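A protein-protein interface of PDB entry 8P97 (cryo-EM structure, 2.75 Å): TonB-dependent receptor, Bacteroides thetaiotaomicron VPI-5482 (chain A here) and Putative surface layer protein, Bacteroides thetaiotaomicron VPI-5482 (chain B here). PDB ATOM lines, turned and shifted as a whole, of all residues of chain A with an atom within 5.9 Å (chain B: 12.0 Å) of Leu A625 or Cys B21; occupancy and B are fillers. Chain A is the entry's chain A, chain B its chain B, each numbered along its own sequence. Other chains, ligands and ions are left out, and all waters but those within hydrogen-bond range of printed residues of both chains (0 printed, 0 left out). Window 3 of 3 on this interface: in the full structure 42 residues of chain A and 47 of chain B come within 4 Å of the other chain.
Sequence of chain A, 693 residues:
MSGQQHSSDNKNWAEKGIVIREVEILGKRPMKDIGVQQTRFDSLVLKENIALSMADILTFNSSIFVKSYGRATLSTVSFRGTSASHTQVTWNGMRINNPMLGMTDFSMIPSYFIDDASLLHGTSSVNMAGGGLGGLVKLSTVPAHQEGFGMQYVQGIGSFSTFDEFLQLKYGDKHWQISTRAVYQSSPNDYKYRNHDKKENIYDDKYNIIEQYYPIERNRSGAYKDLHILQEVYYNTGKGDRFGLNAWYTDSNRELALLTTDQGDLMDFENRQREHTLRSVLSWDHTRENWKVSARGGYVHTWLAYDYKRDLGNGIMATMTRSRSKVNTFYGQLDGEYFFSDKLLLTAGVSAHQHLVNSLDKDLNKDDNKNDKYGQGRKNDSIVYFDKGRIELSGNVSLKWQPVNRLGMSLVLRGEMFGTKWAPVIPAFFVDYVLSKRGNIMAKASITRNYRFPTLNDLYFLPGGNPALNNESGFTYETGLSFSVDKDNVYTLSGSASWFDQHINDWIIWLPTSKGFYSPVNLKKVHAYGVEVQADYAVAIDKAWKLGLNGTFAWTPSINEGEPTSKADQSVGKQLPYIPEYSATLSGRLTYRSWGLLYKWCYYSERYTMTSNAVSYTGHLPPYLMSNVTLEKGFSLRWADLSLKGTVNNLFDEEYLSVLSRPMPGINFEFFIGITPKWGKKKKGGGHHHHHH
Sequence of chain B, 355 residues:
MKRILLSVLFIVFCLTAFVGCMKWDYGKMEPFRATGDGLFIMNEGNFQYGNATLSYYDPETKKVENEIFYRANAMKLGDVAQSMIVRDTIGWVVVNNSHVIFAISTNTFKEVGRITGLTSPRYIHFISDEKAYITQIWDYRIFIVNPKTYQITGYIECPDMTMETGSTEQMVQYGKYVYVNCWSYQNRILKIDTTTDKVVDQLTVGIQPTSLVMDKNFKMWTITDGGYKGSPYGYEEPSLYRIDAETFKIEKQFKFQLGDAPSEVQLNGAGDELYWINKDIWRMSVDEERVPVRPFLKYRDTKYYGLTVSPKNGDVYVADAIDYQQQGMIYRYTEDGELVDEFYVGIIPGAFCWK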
ATOM      1  N   TRP A 601       0.914 -10.105  -8.807  1.00  0.00           N
ATOM      2  CA  TRP A 601       0.804  -8.955  -9.695  1.00  0.00           C
ATOM      3  C   TRP A 601       0.676  -7.690  -8.863  1.00  0.00           C
ATOM      4  O   TRP A 601      -0.117  -7.644  -7.918  1.00  0.00           O
ATOM      5  CB  TRP A 601      -0.393  -9.108 -10.638  1.00  0.00           C
ATOM      6  CG  TRP A 601      -0.659  -7.913 -11.494  1.00  0.00           C
ATOM      7  CD1 TRP A 601       0.046  -7.521 -12.590  1.00  0.00           C
ATOM      8  CD2 TRP A 601      -1.725  -6.971 -11.345  1.00  0.00           C
ATOM      9  NE1 TRP A 601      -0.504  -6.384 -13.125  1.00  0.00           N
ATOM     10  CE2 TRP A 601      -1.594  -6.027 -12.378  1.00  0.00           C
ATOM     11  CE3 TRP A 601      -2.775  -6.830 -10.434  1.00  0.00           C
ATOM     12  CZ2 TRP A 601      -2.470  -4.958 -12.526  1.00  0.00           C
ATOM     13  CZ3 TRP A 601      -3.641  -5.770 -10.584  1.00  0.00           C
ATOM     14  CH2 TRP A 601      -3.485  -4.848 -11.621  1.00  0.00           C
ATOM     15  N   CYS A 602       1.454  -6.669  -9.211  1.00  0.00           N
ATOM     16  CA  CYS A 602       1.456  -5.398  -8.501  1.00  0.00           C
ATOM     17  C   CYS A 602       1.249  -4.260  -9.485  1.00  0.00           C
ATOM     18  O   CYS A 602       1.823  -4.262 -10.576  1.00  0.00           O
ATOM     19  CB  CYS A 602       2.765  -5.188  -7.739  1.00  0.00           C
ATOM     20  SG  CYS A 602       2.831  -3.663  -6.784  1.00  0.00           S
ATOM     21  N   TYR A 603       0.430  -3.288  -9.094  1.00  0.00           N
ATOM     22  CA  TYR A 603       0.143  -2.120  -9.918  1.00  0.00           C
ATOM     23  C   TYR A 603       0.342  -0.857  -9.098  1.00  0.00           C
ATOM     24  O   TYR A 603      -0.232  -0.722  -8.014  1.00  0.00           O
ATOM     25  CB  TYR A 603      -1.280  -2.171 -10.474  1.00  0.00           C
ATOM     26  CG  TYR A 603      -1.705  -0.894 -11.159  1.00  0.00           C
ATOM     27  CD1 TYR A 603      -1.220  -0.560 -12.411  1.00  0.00           C
ATOM     28  CD2 TYR A 603      -2.598  -0.026 -10.554  1.00  0.00           C
ATOM     29  CE1 TYR A 603      -1.606   0.607 -13.035  1.00  0.00           C
ATOM     30  CE2 TYR A 603      -2.991   1.140 -11.171  1.00  0.00           C
ATOM     31  CZ  TYR A 603      -2.492   1.450 -12.409  1.00  0.00           C
ATOM     32  OH  TYR A 603      -2.883   2.613 -13.025  1.00  0.00           O
ATOM     33  N   TYR A 604       1.147   0.062  -9.619  1.00  0.00           N
ATOM     34  CA  TYR A 604       1.296   1.399  -9.068  1.00  0.00           C
ATOM     35  C   TYR A 604       0.990   2.413 -10.157  1.00  0.00           C
ATOM     36  O   TYR A 604       1.430   2.258 -11.298  1.00  0.00           O
ATOM     37  CB  TYR A 604       2.707   1.646  -8.537  1.00  0.00           C
ATOM     38  CG  TYR A 604       3.037   0.921  -7.260  1.00  0.00           C
ATOM     39  CD1 TYR A 604       2.061   0.661  -6.315  1.00  0.00           C
ATOM     40  CD2 TYR A 604       4.332   0.509  -6.994  1.00  0.00           C
ATOM     41  CE1 TYR A 604       2.363   0.003  -5.145  1.00  0.00           C
ATOM     42  CE2 TYR A 604       4.643  -0.149  -5.829  1.00  0.00           C
ATOM     43  CZ  TYR A 604       3.656  -0.399  -4.908  1.00  0.00           C
ATOM     44  OH  TYR A 604       3.963  -1.056  -3.742  1.00  0.00           O
ATOM     45  N   PRO A 623       3.546   4.240 -15.096  1.00  0.00           N
ATOM     46  CA  PRO A 623       2.904   3.353 -14.120  1.00  0.00           C
ATOM     47  C   PRO A 623       3.591   1.998 -14.078  1.00  0.00           C
ATOM     48  O   PRO A 623       4.021   1.467 -15.101  1.00  0.00           O
ATOM     49  CB  PRO A 623       1.464   3.243 -14.632  1.00  0.00           C
ATOM     50  CG  PRO A 623       1.519   3.701 -16.050  1.00  0.00           C
ATOM     51  CD  PRO A 623       2.587   4.735 -16.093  1.00  0.00           C
ATOM     52  N   TYR A 624       3.687   1.440 -12.875  1.00  0.00           N
ATOM     53  CA  TYR A 624       4.504   0.263 -12.608  1.00  0.00           C
ATOM     54  C   TYR A 624       3.616  -0.971 -12.543  1.00  0.00           C
ATOM     55  O   TYR A 624       2.742  -1.064 -11.676  1.00  0.00           O
ATOM     56  CB  TYR A 624       5.277   0.445 -11.304  1.00  0.00           C
ATOM     57  CG  TYR A 624       5.926  -0.803 -10.760  1.00  0.00           C
ATOM     58  CD1 TYR A 624       7.114  -1.276 -11.287  1.00  0.00           C
ATOM     59  CD2 TYR A 624       5.356  -1.500  -9.707  1.00  0.00           C
ATOM     60  CE1 TYR A 624       7.712  -2.411 -10.787  1.00  0.00           C
ATOM     61  CE2 TYR A 624       5.945  -2.637  -9.204  1.00  0.00           C
ATOM     62  CZ  TYR A 624       7.123  -3.087  -9.746  1.00  0.00           C
ATOM     63  OH  TYR A 624       7.716  -4.220  -9.246  1.00  0.00           O
ATOM     64  N   LEU A 625       3.841  -1.913 -13.455  1.00  0.00           N
ATOM     65  CA  LEU A 625       3.125  -3.183 -13.481  1.00  0.00           C
ATOM     66  C   LEU A 625       4.148  -4.306 -13.528  1.00  0.00           C
ATOM     67  O   LEU A 625       5.027  -4.309 -14.395  1.00  0.00           O
ATOM     68  CB  LEU A 625       2.183  -3.272 -14.683  1.00  0.00           C
ATOM     69  CG  LEU A 625       0.889  -2.455 -14.671  1.00  0.00           C
ATOM     70  CD1 LEU A 625       1.154  -0.995 -14.979  1.00  0.00           C
ATOM     71  CD2 LEU A 625      -0.115  -3.025 -15.645  1.00  0.00           C
ATOM     72  N   MET A 626       4.036  -5.256 -12.603  1.00  0.00           N
ATOM     73  CA  MET A 626       4.973  -6.366 -12.513  1.00  0.00           C
ATOM     74  C   MET A 626       4.224  -7.663 -12.254  1.00  0.00           C
ATOM     75  O   MET A 626       3.168  -7.673 -11.616  1.00  0.00           O
ATOM     76  CB  MET A 626       6.014  -6.126 -11.417  1.00  0.00           C
ATOM     77  CG  MET A 626       7.090  -7.186 -11.345  1.00  0.00           C
ATOM     78  SD  MET A 626       8.064  -7.225 -12.852  1.00  0.00           S
ATOM     79  CE  MET A 626       8.997  -5.719 -12.666  1.00  0.00           C
ATOM     80  N   SER A 627       4.782  -8.760 -12.759  1.00  0.00           N
ATOM     81  CA  SER A 627       4.161 -10.073 -12.666  1.00  0.00           C
ATOM     82  C   SER A 627       5.214 -11.117 -12.327  1.00  0.00           C
ATOM     83  O   SER A 627       6.240 -11.203 -13.007  1.00  0.00           O
ATOM     84  CB  SER A 627       3.463 -10.429 -13.979  1.00  0.00           C
ATOM     85  OG  SER A 627       2.744 -11.635 -13.854  1.00  0.00           O
ATOM     86  N   PHE A 652       7.268 -10.944 -18.057  1.00  0.00           N
ATOM     87  CA  PHE A 652       7.095 -10.412 -19.400  1.00  0.00           C
ATOM     88  C   PHE A 652       8.322  -9.676 -19.918  1.00  0.00           C
ATOM     89  O   PHE A 652       8.279  -9.149 -21.032  1.00  0.00           O
ATOM     90  CB  PHE A 652       5.880  -9.485 -19.441  1.00  0.00           C
ATOM     91  CG  PHE A 652       4.579 -10.197 -19.234  1.00  0.00           C
ATOM     92  CD1 PHE A 652       3.934 -10.805 -20.291  1.00  0.00           C
ATOM     93  CD2 PHE A 652       4.006 -10.262 -17.981  1.00  0.00           C
ATOM     94  CE1 PHE A 652       2.742 -11.466 -20.100  1.00  0.00           C
ATOM     95  CE2 PHE A 652       2.812 -10.919 -17.787  1.00  0.00           C
ATOM     96  CZ  PHE A 652       2.181 -11.522 -18.846  1.00  0.00           C
ATOM     97  N   GLU A 654      10.108  -6.752 -18.985  1.00  0.00           N
ATOM     98  CA  GLU A 654       9.981  -5.321 -19.209  1.00  0.00           C
ATOM     99  C   GLU A 654      11.323  -4.626 -19.033  1.00  0.00           C
ATOM    100  O   GLU A 654      12.092  -4.945 -18.122  1.00  0.00           O
ATOM    101  CB  GLU A 654       8.960  -4.708 -18.253  1.00  0.00           C
ATOM    102  CG  GLU A 654       7.540  -4.680 -18.778  1.00  0.00           C
ATOM    103  CD  GLU A 654       6.756  -5.918 -18.417  1.00  0.00           C
ATOM    104  OE1 GLU A 654       7.126  -6.592 -17.436  1.00  0.00           O
ATOM    105  OE2 GLU A 654       5.764  -6.214 -19.110  1.00  0.00           O
ATOM    106  N   CYS B  21      -0.382  -4.071 -20.233  1.00  0.00           N
ATOM    107  CA  CYS B  21       0.269  -4.477 -18.994  1.00  0.00           C
ATOM    108  C   CYS B  21       1.781  -4.542 -19.168  1.00  0.00           C
ATOM    109  O   CYS B  21       2.420  -5.500 -18.739  1.00  0.00           O
ATOM    110  CB  CYS B  21      -0.269  -5.831 -18.527  1.00  0.00           C
ATOM    111  SG  CYS B  21      -1.999  -5.801 -18.014  1.00  0.00           S
ATOM    112  N   MET B  22       2.350  -3.517 -19.799  1.00  0.00           N
ATOM    113  CA  MET B  22       3.775  -3.482 -20.091  1.00  0.00           C
ATOM    114  C   MET B  22       4.286  -2.056 -19.950  1.00  0.00           C
ATOM    115  O   MET B  22       3.515  -1.096 -19.914  1.00  0.00           O
ATOM    116  CB  MET B  22       4.076  -4.030 -21.492  1.00  0.00           C
ATOM    117  CG  MET B  22       3.798  -5.516 -21.632  1.00  0.00           C
ATOM    118  SD  MET B  22       4.134  -6.184 -23.266  1.00  0.00           S
ATOM    119  CE  MET B  22       3.597  -7.876 -23.031  1.00  0.00           C
ATOM    120  N   LYS B  23       5.610  -1.934 -19.860  1.00  0.00           N
ATOM    121  CA  LYS B  23       6.283  -0.669 -19.604  1.00  0.00           C
ATOM    122  C   LYS B  23       7.432  -0.498 -20.592  1.00  0.00           C
ATOM    123  O   LYS B  23       7.933  -1.469 -21.162  1.00  0.00           O
ATOM    124  CB  LYS B  23       6.777  -0.608 -18.151  1.00  0.00           C
ATOM    125  CG  LYS B  23       5.708  -1.047 -17.153  1.00  0.00           C
ATOM    126  CD  LYS B  23       6.100  -0.818 -15.708  1.00  0.00           C
ATOM    127  CE  LYS B  23       7.230  -1.720 -15.283  1.00  0.00           C
ATOM    128  NZ  LYS B  23       6.994  -3.125 -15.689  1.00  0.00           N
ATOM    129  N   TRP B  24       7.843   0.754 -20.798  1.00  0.00           N
ATOM    130  CA  TRP B  24       8.760   1.084 -21.887  1.00  0.00           C
ATOM    131  C   TRP B  24       9.320   2.490 -21.702  1.00  0.00           C
ATOM    132  O   TRP B  24       8.715   3.330 -21.031  1.00  0.00           O
ATOM    133  CB  TRP B  24       8.050   0.952 -23.239  1.00  0.00           C
ATOM    134  CG  TRP B  24       7.357   2.202 -23.681  1.00  0.00           C
ATOM    135  CD1 TRP B  24       6.097   2.597 -23.340  1.00  0.00           C
ATOM    136  CD2 TRP B  24       7.860   3.200 -24.578  1.00  0.00           C
ATOM    137  NE1 TRP B  24       5.791   3.788 -23.948  1.00  0.00           N
ATOM    138  CE2 TRP B  24       6.855   4.179 -24.716  1.00  0.00           C
ATOM    139  CE3 TRP B  24       9.063   3.367 -25.269  1.00  0.00           C
ATOM    140  CZ2 TRP B  24       7.019   5.307 -25.516  1.00  0.00           C
ATOM    141  CZ3 TRP B  24       9.219   4.487 -26.063  1.00  0.00           C
ATOM    142  CH2 TRP B  24       8.205   5.443 -26.180  1.00  0.00           C
ATOM    143  N   ASP B  25      10.489   2.730 -22.307  1.00  0.00           N
ATOM    144  CA  ASP B  25      11.101   4.055 -22.347  1.00  0.00           C
ATOM    145  C   ASP B  25      12.173   4.126 -23.432  1.00  0.00           C
ATOM    146  O   ASP B  25      13.183   3.422 -23.363  1.00  0.00           O
ATOM    147  CB  ASP B  25      11.709   4.446 -20.989  1.00  0.00           C
ATOM    148  CG  ASP B  25      12.690   3.411 -20.454  1.00  0.00           C
ATOM    149  OD1 ASP B  25      12.765   2.301 -21.015  1.00  0.00           O
ATOM    150  OD2 ASP B  25      13.413   3.725 -19.485  1.00  0.00           O
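Pro A623 touches Lys B23 (O to CD, 3.1 Å). Lys B23 touches Tyr A624. CD2 of Leu A625 touches CA of Cys B21, 3.7 Å away. Glu A654 touches Met B22 (OE2 to CG, 3.3 Å).
The backbone NH of Tyr A604 is in hydrogen-bond range of the backbone carbonyl oxygen of Tyr A624 (2.8 Å).
Of chain B, only Cys B21 and Lys B23 come within 4 Å of Leu A625. Of chain A, only Leu A625 and Glu A654 come within 4 Å of Cys B21. Cys A602 touches none of the printed residues of chain B. Tyr A624 touches one residue of chain B. No residue of chain B comes within 4 Å of Ser A627. No residue of chain B comes within 4 Å of Phe A652. Printed residues of chain A within 4 Å of Met B22: Glu A654. Of the printed residues of chain A, Lys B23 touches Pro A623 (3.1 Å), Tyr A624 (3.7 Å), Leu A625 (2.6 Å) and Glu A654 (3.5 Å). Printed residues of chain B within 4 Å of Glu A654: Cys B21, Met B22 and Lys B23. Trp B24 touches none of the printed residues of chain A. The nearest residue of chain B that does not touch Leu A625 is Met B22 (4.9 Å). The nearest residue of chain A that does not touch Cys B21 is Phe A652 (5.1 Å).
NZ of Lys B23 lies within hydrogen-bond range of O of Leu A625, at 2.6 Å. The side-chain carboxylate (OE1) of Glu A654 is in salt-bridge range of the side-chain amino group (NZ) of Lys B23 (3.9 Å). OE2 of Glu A654 lies close to O of Cys B21 (3.4 Å).
Hydrophobic or aromatic side chains of chain B within 4 Å of the printed part of chain A: Met B22. Printed residues of chain A that touch a printed residue of chain B: Pro A623, Tyr A624, Leu A625 and Glu A654. Hydrophobic or aromatic side chains of chain A within 4 Å of the printed part of chain B: Leu A625. Along chain A the printed residues that touch a printed residue of chain B span positions 623 to 654. Among the printed residues, 7 pairs touch across the chains.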
